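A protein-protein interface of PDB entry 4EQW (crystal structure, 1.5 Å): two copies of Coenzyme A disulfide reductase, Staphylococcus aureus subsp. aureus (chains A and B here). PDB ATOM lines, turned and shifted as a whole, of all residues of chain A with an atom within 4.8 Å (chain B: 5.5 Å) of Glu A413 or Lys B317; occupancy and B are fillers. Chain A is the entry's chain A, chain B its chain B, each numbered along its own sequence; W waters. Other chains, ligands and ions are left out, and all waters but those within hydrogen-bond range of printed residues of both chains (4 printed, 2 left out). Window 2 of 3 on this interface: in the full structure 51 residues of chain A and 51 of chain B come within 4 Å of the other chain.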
ATOM      1  N   GLU A 410       6.048  -9.890   0.737  1.00  0.00           N
ATOM      2  CA  GLU A 410       5.155 -10.960   0.291  1.00  0.00           C
ATOM      3  C   GLU A 410       3.918 -11.117   1.173  1.00  0.00           C
ATOM      4  O   GLU A 410       3.008 -11.872   0.834  1.00  0.00           O
ATOM      5  CB  GLU A 410       5.906 -12.290   0.198  1.00  0.00           C
ATOM      6  CG  GLU A 410       6.902 -12.343  -0.959  1.00  0.00           C
ATOM      7  CD  GLU A 410       7.793 -13.567  -0.896  1.00  0.00           C
ATOM      8  OE1 GLU A 410       8.694 -13.606  -0.031  1.00  0.00           O
ATOM      9  OE2 GLU A 410       7.595 -14.486  -1.717  1.00  0.00           O
ATOM     10  N   LEU A 411       3.875 -10.407   2.298  1.00  0.00           N
ATOM     11  CA  LEU A 411       2.708 -10.492   3.170  1.00  0.00           C
ATOM     12  C   LEU A 411       1.462  -9.909   2.496  1.00  0.00           C
ATOM     13  O   LEU A 411       0.339 -10.225   2.890  1.00  0.00           O
ATOM     14  CB  LEU A 411       2.982  -9.824   4.526  1.00  0.00           C
ATOM     15  CG  LEU A 411       4.065 -10.483   5.387  1.00  0.00           C
ATOM     16  CD1 LEU A 411       4.313  -9.667   6.649  1.00  0.00           C
ATOM     17  CD2 LEU A 411       3.677 -11.918   5.755  1.00  0.00           C
ATOM     18  N   THR A 412       1.649  -9.071   1.481  1.00  0.00           N
ATOM     19  CA  THR A 412       0.498  -8.558   0.743  1.00  0.00           C
ATOM     20  C   THR A 412      -0.255  -9.693   0.047  1.00  0.00           C
ATOM     21  O   THR A 412      -1.445  -9.563  -0.265  1.00  0.00           O
ATOM     22  CB  THR A 412       0.910  -7.531  -0.336  1.00  0.00           C
ATOM     23  OG1 THR A 412       1.823  -8.146  -1.253  1.00  0.00           O
ATOM     24  CG2 THR A 412       1.572  -6.313   0.295  1.00  0.00           C
ATOM     25  N   GLU A 413       0.442 -10.802  -0.180  1.00  0.00           N
ATOM     26  CA  GLU A 413      -0.088 -11.936  -0.939  1.00  0.00           C
ATOM     27  C   GLU A 413      -0.794 -12.972  -0.065  1.00  0.00           C
ATOM     28  O   GLU A 413      -1.418 -13.905  -0.580  1.00  0.00           O
ATOM     29  CB  GLU A 413       1.042 -12.623  -1.716  1.00  0.00           C
ATOM     30  CG  GLU A 413       1.787 -11.709  -2.687  1.00  0.00           C
ATOM     31  CD  GLU A 413       3.054 -12.342  -3.214  1.00  0.00           C
ATOM     32  OE1 GLU A 413       3.234 -13.554  -3.006  1.00  0.00           O
ATOM     33  OE2 GLU A 413       3.869 -11.628  -3.835  1.00  0.00           O
ATOM     34  N   PHE A 414      -0.678 -12.823   1.251  1.00  0.00           N
ATOM     35  CA  PHE A 414      -1.324 -13.752   2.167  1.00  0.00           C
ATOM     36  C   PHE A 414      -2.838 -13.703   1.980  1.00  0.00           C
ATOM     37  O   PHE A 414      -3.443 -12.634   2.044  1.00  0.00           O
ATOM     38  CB  PHE A 414      -0.942 -13.420   3.614  1.00  0.00           C
ATOM     39  CG  PHE A 414      -1.796 -14.113   4.636  1.00  0.00           C
ATOM     40  CD1 PHE A 414      -1.817 -15.497   4.720  1.00  0.00           C
ATOM     41  CD2 PHE A 414      -2.578 -13.371   5.513  1.00  0.00           C
ATOM     42  CE1 PHE A 414      -2.605 -16.134   5.667  1.00  0.00           C
ATOM     43  CE2 PHE A 414      -3.367 -14.003   6.463  1.00  0.00           C
ATOM     44  CZ  PHE A 414      -3.388 -15.381   6.529  1.00  0.00           C
ATOM     45  N   GLU A 415      -3.433 -14.866   1.741  1.00  0.00           N
ATOM     46  CA  GLU A 415      -4.865 -14.970   1.493  1.00  0.00           C
ATOM     47  C   GLU A 415      -5.557 -15.405   2.779  1.00  0.00           C
ATOM     48  O   GLU A 415      -5.546 -16.584   3.147  1.00  0.00           O
ATOM     49  CB  GLU A 415      -5.139 -15.945   0.344  1.00  0.00           C
ATOM     50  CG  GLU A 415      -6.607 -15.977  -0.067  1.00  0.00           C
ATOM     51  CD  GLU A 415      -6.870 -16.820  -1.295  1.00  0.00           C
ATOM     52  OE1 GLU A 415      -7.990 -17.360  -1.394  1.00  0.00           O
ATOM     53  OE2 GLU A 415      -5.974 -16.942  -2.156  1.00  0.00           O
ATOM     54  N   ASN A 430      -1.741  -8.489   5.810  1.00  0.00           N
ATOM     55  CA  ASN A 430      -1.630  -7.833   4.509  1.00  0.00           C
ATOM     56  C   ASN A 430      -1.179  -6.376   4.646  1.00  0.00           C
ATOM     57  O   ASN A 430      -0.326  -5.910   3.895  1.00  0.00           O
ATOM     58  CB  ASN A 430      -2.967  -7.867   3.757  1.00  0.00           C
ATOM     59  CG  ASN A 430      -3.466  -9.281   3.473  1.00  0.00           C
ATOM     60  OD1 ASN A 430      -4.652  -9.576   3.665  1.00  0.00           O
ATOM     61  ND2 ASN A 430      -2.591 -10.144   2.966  1.00  0.00           N
ATOM     62  N   ASP B 262      -2.577 -12.388 -15.142  1.00  0.00           N
ATOM     63  CA  ASP B 262      -2.136 -12.081 -13.784  1.00  0.00           C
ATOM     64  C   ASP B 262      -2.053 -10.582 -13.488  1.00  0.00           C
ATOM     65  O   ASP B 262      -1.806 -10.185 -12.351  1.00  0.00           O
ATOM     66  CB  ASP B 262      -0.802 -12.769 -13.473  1.00  0.00           C
ATOM     67  CG  ASP B 262      -0.941 -14.269 -13.316  1.00  0.00           C
ATOM     68  OD1 ASP B 262      -2.071 -14.753 -13.125  1.00  0.00           O
ATOM     69  OD2 ASP B 262       0.087 -14.967 -13.385  1.00  0.00           O
ATOM     70  N   HIS B 281      -6.567 -18.504 -11.854  1.00  0.00           N
ATOM     71  CA  HIS B 281      -6.066 -19.855 -11.619  1.00  0.00           C
ATOM     72  C   HIS B 281      -5.689 -20.004 -10.155  1.00  0.00           C
ATOM     73  O   HIS B 281      -5.514 -19.015  -9.447  1.00  0.00           O
ATOM     74  CB  HIS B 281      -4.832 -20.127 -12.482  1.00  0.00           C
ATOM     75  CG  HIS B 281      -3.742 -19.120 -12.291  1.00  0.00           C
ATOM     76  ND1 HIS B 281      -2.751 -19.266 -11.347  1.00  0.00           N
ATOM     77  CD2 HIS B 281      -3.503 -17.938 -12.910  1.00  0.00           C
ATOM     78  CE1 HIS B 281      -1.943 -18.222 -11.394  1.00  0.00           C
ATOM     79  NE2 HIS B 281      -2.376 -17.402 -12.334  1.00  0.00           N
ATOM     80  N   TYR B 282      -5.582 -21.245  -9.705  1.00  0.00           N
ATOM     81  CA  TYR B 282      -5.032 -21.515  -8.389  1.00  0.00           C
ATOM     82  C   TYR B 282      -3.546 -21.170  -8.326  1.00  0.00           C
ATOM     83  O   TYR B 282      -2.816 -21.242  -9.327  1.00  0.00           O
ATOM     84  CB  TYR B 282      -5.241 -22.980  -8.000  1.00  0.00           C
ATOM     85  CG  TYR B 282      -6.656 -23.326  -7.591  1.00  0.00           C
ATOM     86  CD1 TYR B 282      -7.486 -24.076  -8.426  1.00  0.00           C
ATOM     87  CD2 TYR B 282      -7.166 -22.906  -6.367  1.00  0.00           C
ATOM     88  CE1 TYR B 282      -8.785 -24.396  -8.044  1.00  0.00           C
ATOM     89  CE2 TYR B 282      -8.459 -23.218  -5.980  1.00  0.00           C
ATOM     90  CZ  TYR B 282      -9.265 -23.961  -6.821  1.00  0.00           C
ATOM     91  OH  TYR B 282     -10.544 -24.276  -6.413  1.00  0.00           O
ATOM     92  N   ARG B 283      -3.098 -20.817  -7.127  1.00  0.00           N
ATOM     93  CA  ARG B 283      -1.694 -20.528  -6.898  1.00  0.00           C
ATOM     94  C   ARG B 283      -0.868 -21.809  -6.768  1.00  0.00           C
ATOM     95  O   ARG B 283       0.281 -21.862  -7.213  1.00  0.00           O
ATOM     96  CB  ARG B 283      -1.521 -19.658  -5.647  1.00  0.00           C
ATOM     97  CG  ARG B 283      -0.066 -19.461  -5.262  1.00  0.00           C
ATOM     98  CD  ARG B 283       0.121 -18.375  -4.211  1.00  0.00           C
ATOM     99  NE  ARG B 283       1.545 -18.199  -3.942  1.00  0.00           N
ATOM    100  CZ  ARG B 283       2.110 -17.066  -3.532  1.00  0.00           C
ATOM    101  NH1 ARG B 283       1.384 -15.979  -3.331  1.00  0.00           N
ATOM    102  NH2 ARG B 283       3.420 -17.018  -3.329  1.00  0.00           N
ATOM    103  N   TRP B 295     -11.669 -10.960  -0.242  1.00  0.00           N
ATOM    104  CA  TRP B 295     -10.209 -10.902  -0.305  1.00  0.00           C
ATOM    105  C   TRP B 295      -9.729 -10.699  -1.734  1.00  0.00           C
ATOM    106  O   TRP B 295      -8.876  -9.847  -1.992  1.00  0.00           O
ATOM    107  CB  TRP B 295      -9.543 -12.153   0.301  1.00  0.00           C
ATOM    108  CG  TRP B 295      -8.045 -12.058   0.242  1.00  0.00           C
ATOM    109  CD1 TRP B 295      -7.225 -11.506   1.179  1.00  0.00           C
ATOM    110  CD2 TRP B 295      -7.199 -12.479  -0.838  1.00  0.00           C
ATOM    111  NE1 TRP B 295      -5.913 -11.572   0.757  1.00  0.00           N
ATOM    112  CE2 TRP B 295      -5.871 -12.168  -0.475  1.00  0.00           C
ATOM    113  CE3 TRP B 295      -7.434 -13.111  -2.059  1.00  0.00           C
ATOM    114  CZ2 TRP B 295      -4.781 -12.454  -1.305  1.00  0.00           C
ATOM    115  CZ3 TRP B 295      -6.357 -13.393  -2.885  1.00  0.00           C
ATOM    116  CH2 TRP B 295      -5.047 -13.065  -2.505  1.00  0.00           C
ATOM    117  N   ARG B 299      -7.680  -7.649  -3.322  1.00  0.00           N
ATOM    118  CA  ARG B 299      -6.320  -7.882  -3.787  1.00  0.00           C
ATOM    119  C   ARG B 299      -6.196  -7.468  -5.250  1.00  0.00           C
ATOM    120  O   ARG B 299      -5.226  -6.813  -5.636  1.00  0.00           O
ATOM    121  CB  ARG B 299      -5.910  -9.348  -3.585  1.00  0.00           C
ATOM    122  CG  ARG B 299      -4.505  -9.670  -4.106  1.00  0.00           C
ATOM    123  CD  ARG B 299      -3.420  -8.888  -3.344  1.00  0.00           C
ATOM    124  NE  ARG B 299      -2.123  -9.057  -3.994  1.00  0.00           N
ATOM    125  CZ  ARG B 299      -1.153  -8.152  -3.997  1.00  0.00           C
ATOM    126  NH1 ARG B 299      -0.015  -8.398  -4.653  1.00  0.00           N
ATOM    127  NH2 ARG B 299      -1.322  -7.001  -3.366  1.00  0.00           N
ATOM    128  N   GLU B 315       2.212  -8.550  -9.941  1.00  0.00           N
ATOM    129  CA  GLU B 315       1.217  -9.418 -10.571  1.00  0.00           C
ATOM    130  C   GLU B 315       0.608 -10.434  -9.599  1.00  0.00           C
ATOM    131  O   GLU B 315       1.233 -10.822  -8.610  1.00  0.00           O
ATOM    132  CB  GLU B 315       1.821 -10.149 -11.775  1.00  0.00           C
ATOM    133  CG  GLU B 315       2.319  -9.204 -12.868  1.00  0.00           C
ATOM    134  CD  GLU B 315       2.651  -9.910 -14.172  1.00  0.00           C
ATOM    135  OE1 GLU B 315       2.215 -11.063 -14.368  1.00  0.00           O
ATOM    136  OE2 GLU B 315       3.345  -9.300 -15.012  1.00  0.00           O
ATOM    137  N   PHE B 316      -0.618 -10.860  -9.898  1.00  0.00           N
ATOM    138  CA  PHE B 316      -1.325 -11.880  -9.129  1.00  0.00           C
ATOM    139  C   PHE B 316      -0.565 -13.190  -9.203  1.00  0.00           C
ATOM    140  O   PHE B 316       0.029 -13.516 -10.233  1.00  0.00           O
ATOM    141  CB  PHE B 316      -2.717 -12.072  -9.741  1.00  0.00           C
ATOM    142  CG  PHE B 316      -3.707 -12.800  -8.851  1.00  0.00           C
ATOM    143  CD1 PHE B 316      -3.875 -12.452  -7.516  1.00  0.00           C
ATOM    144  CD2 PHE B 316      -4.517 -13.793  -9.384  1.00  0.00           C
ATOM    145  CE1 PHE B 316      -4.815 -13.114  -6.727  1.00  0.00           C
ATOM    146  CE2 PHE B 316      -5.457 -14.455  -8.601  1.00  0.00           C
ATOM    147  CZ  PHE B 316      -5.606 -14.116  -7.279  1.00  0.00           C
ATOM    148  N   LYS B 317      -0.592 -13.960  -8.122  1.00  0.00           N
ATOM    149  CA  LYS B 317       0.052 -15.261  -8.149  1.00  0.00           C
ATOM    150  C   LYS B 317      -0.961 -16.404  -8.075  1.00  0.00           C
ATOM    151  O   LYS B 317      -0.585 -17.567  -7.948  1.00  0.00           O
ATOM    152  CB  LYS B 317       1.124 -15.361  -7.058  1.00  0.00           C
ATOM    153  CG  LYS B 317       2.354 -14.521  -7.404  1.00  0.00           C
ATOM    154  CD  LYS B 317       3.358 -14.437  -6.278  1.00  0.00           C
ATOM    155  CE  LYS B 317       4.532 -13.561  -6.696  1.00  0.00           C
ATOM    156  NZ  LYS B 317       5.386 -13.164  -5.541  1.00  0.00           N
ATOM    157  N   GLY B 318      -2.246 -16.073  -8.189  1.00  0.00           N
ATOM    158  CA  GLY B 318      -3.275 -17.095  -8.163  1.00  0.00           C
ATOM    159  C   GLY B 318      -4.041 -17.166  -6.851  1.00  0.00           C
ATOM    160  O   GLY B 318      -3.614 -16.594  -5.844  1.00  0.00           O
ATOM    161  N   PHE B 319      -5.160 -17.885  -6.867  1.00  0.00           N
ATOM    162  CA  PHE B 319      -6.023 -18.041  -5.697  1.00  0.00           C
ATOM    163  C   PHE B 319      -5.688 -19.299  -4.910  1.00  0.00           C
ATOM    164  O   PHE B 319      -5.266 -20.310  -5.477  1.00  0.00           O
ATOM    165  CB  PHE B 319      -7.486 -18.163  -6.124  1.00  0.00           C
ATOM    166  CG  PHE B 319      -8.140 -16.859  -6.478  1.00  0.00           C
ATOM    167  CD1 PHE B 319      -8.483 -16.581  -7.787  1.00  0.00           C
ATOM    168  CD2 PHE B 319      -8.443 -15.933  -5.496  1.00  0.00           C
ATOM    169  CE1 PHE B 319      -9.098 -15.386  -8.116  1.00  0.00           C
ATOM    170  CE2 PHE B 319      -9.066 -14.745  -5.817  1.00  0.00           C
ATOM    171  CZ  PHE B 319      -9.391 -14.475  -7.119  1.00  0.00           C
ATOM    172  N   MET B 403       0.956 -21.272   0.317  1.00  0.00           N
ATOM    173  CA  MET B 403       1.582 -20.158  -0.385  1.00  0.00           C
ATOM    174  C   MET B 403       3.081 -20.434  -0.561  1.00  0.00           C
ATOM    175  O   MET B 403       3.711 -19.964  -1.510  1.00  0.00           O
ATOM    176  CB  MET B 403       1.377 -18.887   0.449  1.00  0.00           C
ATOM    177  CG  MET B 403       1.430 -17.571  -0.292  1.00  0.00           C
ATOM    178  SD  MET B 403       1.537 -16.219   0.910  1.00  0.00           S
ATOM    179  CE  MET B 403       3.309 -16.034   1.019  1.00  0.00           C
HETATM  180  O   HOH W   1      -1.823 -17.325   1.701  1.00  0.00           O
HETATM  181  O   HOH W   2       5.392 -14.927  -3.380  1.00  0.00           O
HETATM  182  O   HOH W   3       2.429  -6.757  -3.688  1.00  0.00           O
HETATM  183  O   HOH W   4      -3.437 -16.566  -3.114  1.00  0.00           O
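NZ of Lys B317 is in salt-bridge range of OE2 of Glu A413 (2.8 Å). O of Phe A414 sits at hydrogen-bond distance from NE1 of Trp B295, at 3.0 Å. The guanidinium group of Arg B283 is in salt-bridge range of the side-chain carboxylate of Glu A413 (3.1 Å).
Printed residues of chain A that touch a printed residue of chain B: Thr A412, Glu A413, Phe A414, Glu A415 and Asn A430. Of the 12 printed residues of chain B, 6 touch a printed residue of chain A. Hydrophobic or aromatic side chains of chain B within 4 Å of the printed part of chain A: Trp B295 and Met B403. Among the printed residues, Asp or Glu carboxylates within 4 Å of a Lys or Arg side-chain nitrogen of the other chain: Glu A413 with Arg B283 (3.1 Å) and Glu A413 with Lys B317 (2.8 Å).
Water W2 lies within hydrogen-bond range of the side-chain carboxylate (OE1) of Glu A413 (2.6 Å), the side-chain amino group (NZ) of Lys B317 (2.8 Å), the side-chain carboxylate (OE2) of Glu A410 (2.8 Å) and the guanidinium group (NH2) of Arg B283 (2.9 Å). Water W4 lies within hydrogen-bond range of O of Gly B318 and OE2 of Glu A415. Water W3 bridges the side-chain hydroxyl of Thr A412 (2.9 Å) and the guanidinium group of Arg B299 (3.1 Å). Water W1 lies within hydrogen-bond range of N of Glu A415 (2.9 Å) and SD of Met B403 (3.6 Å).
No position is printed for both chains. Of the 9 pairs that touch across the chains among the printed residues, none has its exchanged pair printed and touching as well.
N of Phe B319 sits at hydrogen-bond distance from O of His B281 (2.8 Å). O of Thr A412 is in hydrogen-bond range of ND2 of Asn A430 (3.5 Å). The backbone carbonyl oxygen (O) of Phe A414 sits at hydrogen-bond distance from the side-chain amide nitrogen (ND2) of Asn A430 (2.8 Å). The backbone NH of Arg B283 sits at hydrogen-bond distance from the backbone carbonyl oxygen of Phe B319 (2.8 Å). NH2 of Arg B283 lies within hydrogen-bond range of O of Met B403, at 3.5 Å. The side-chain amide nitrogen (ND2) of Asn A430 is in hydrogen-bond range of the backbone carbonyl oxygen (O) of Leu A411, at 2.9 Å.
Of chain B, only Arg B283, Trp B295 and Lys B317 come within 4 Å of Glu A413. Of the printed residues of chain B, Glu A415 touches Trp B295 (3.6 Å) and Phe B319 (3.6 Å). Of the printed residues of chain B, Asn A430 touches Trp B295. Lys B317 touches just one residue of chain A: Glu A413. Of the printed residues of chain A, Phe B319 touches Glu A415 (3.6 Å).
Among the printed residues, pairs that only touch across the chains: Thr A412 with Arg B299, Glu A413 with Trp B295, Phe A414 with Met B403, Glu A415 with Trp B295, Glu A415 with Phe B319 and Asn A430 with Trp B295.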
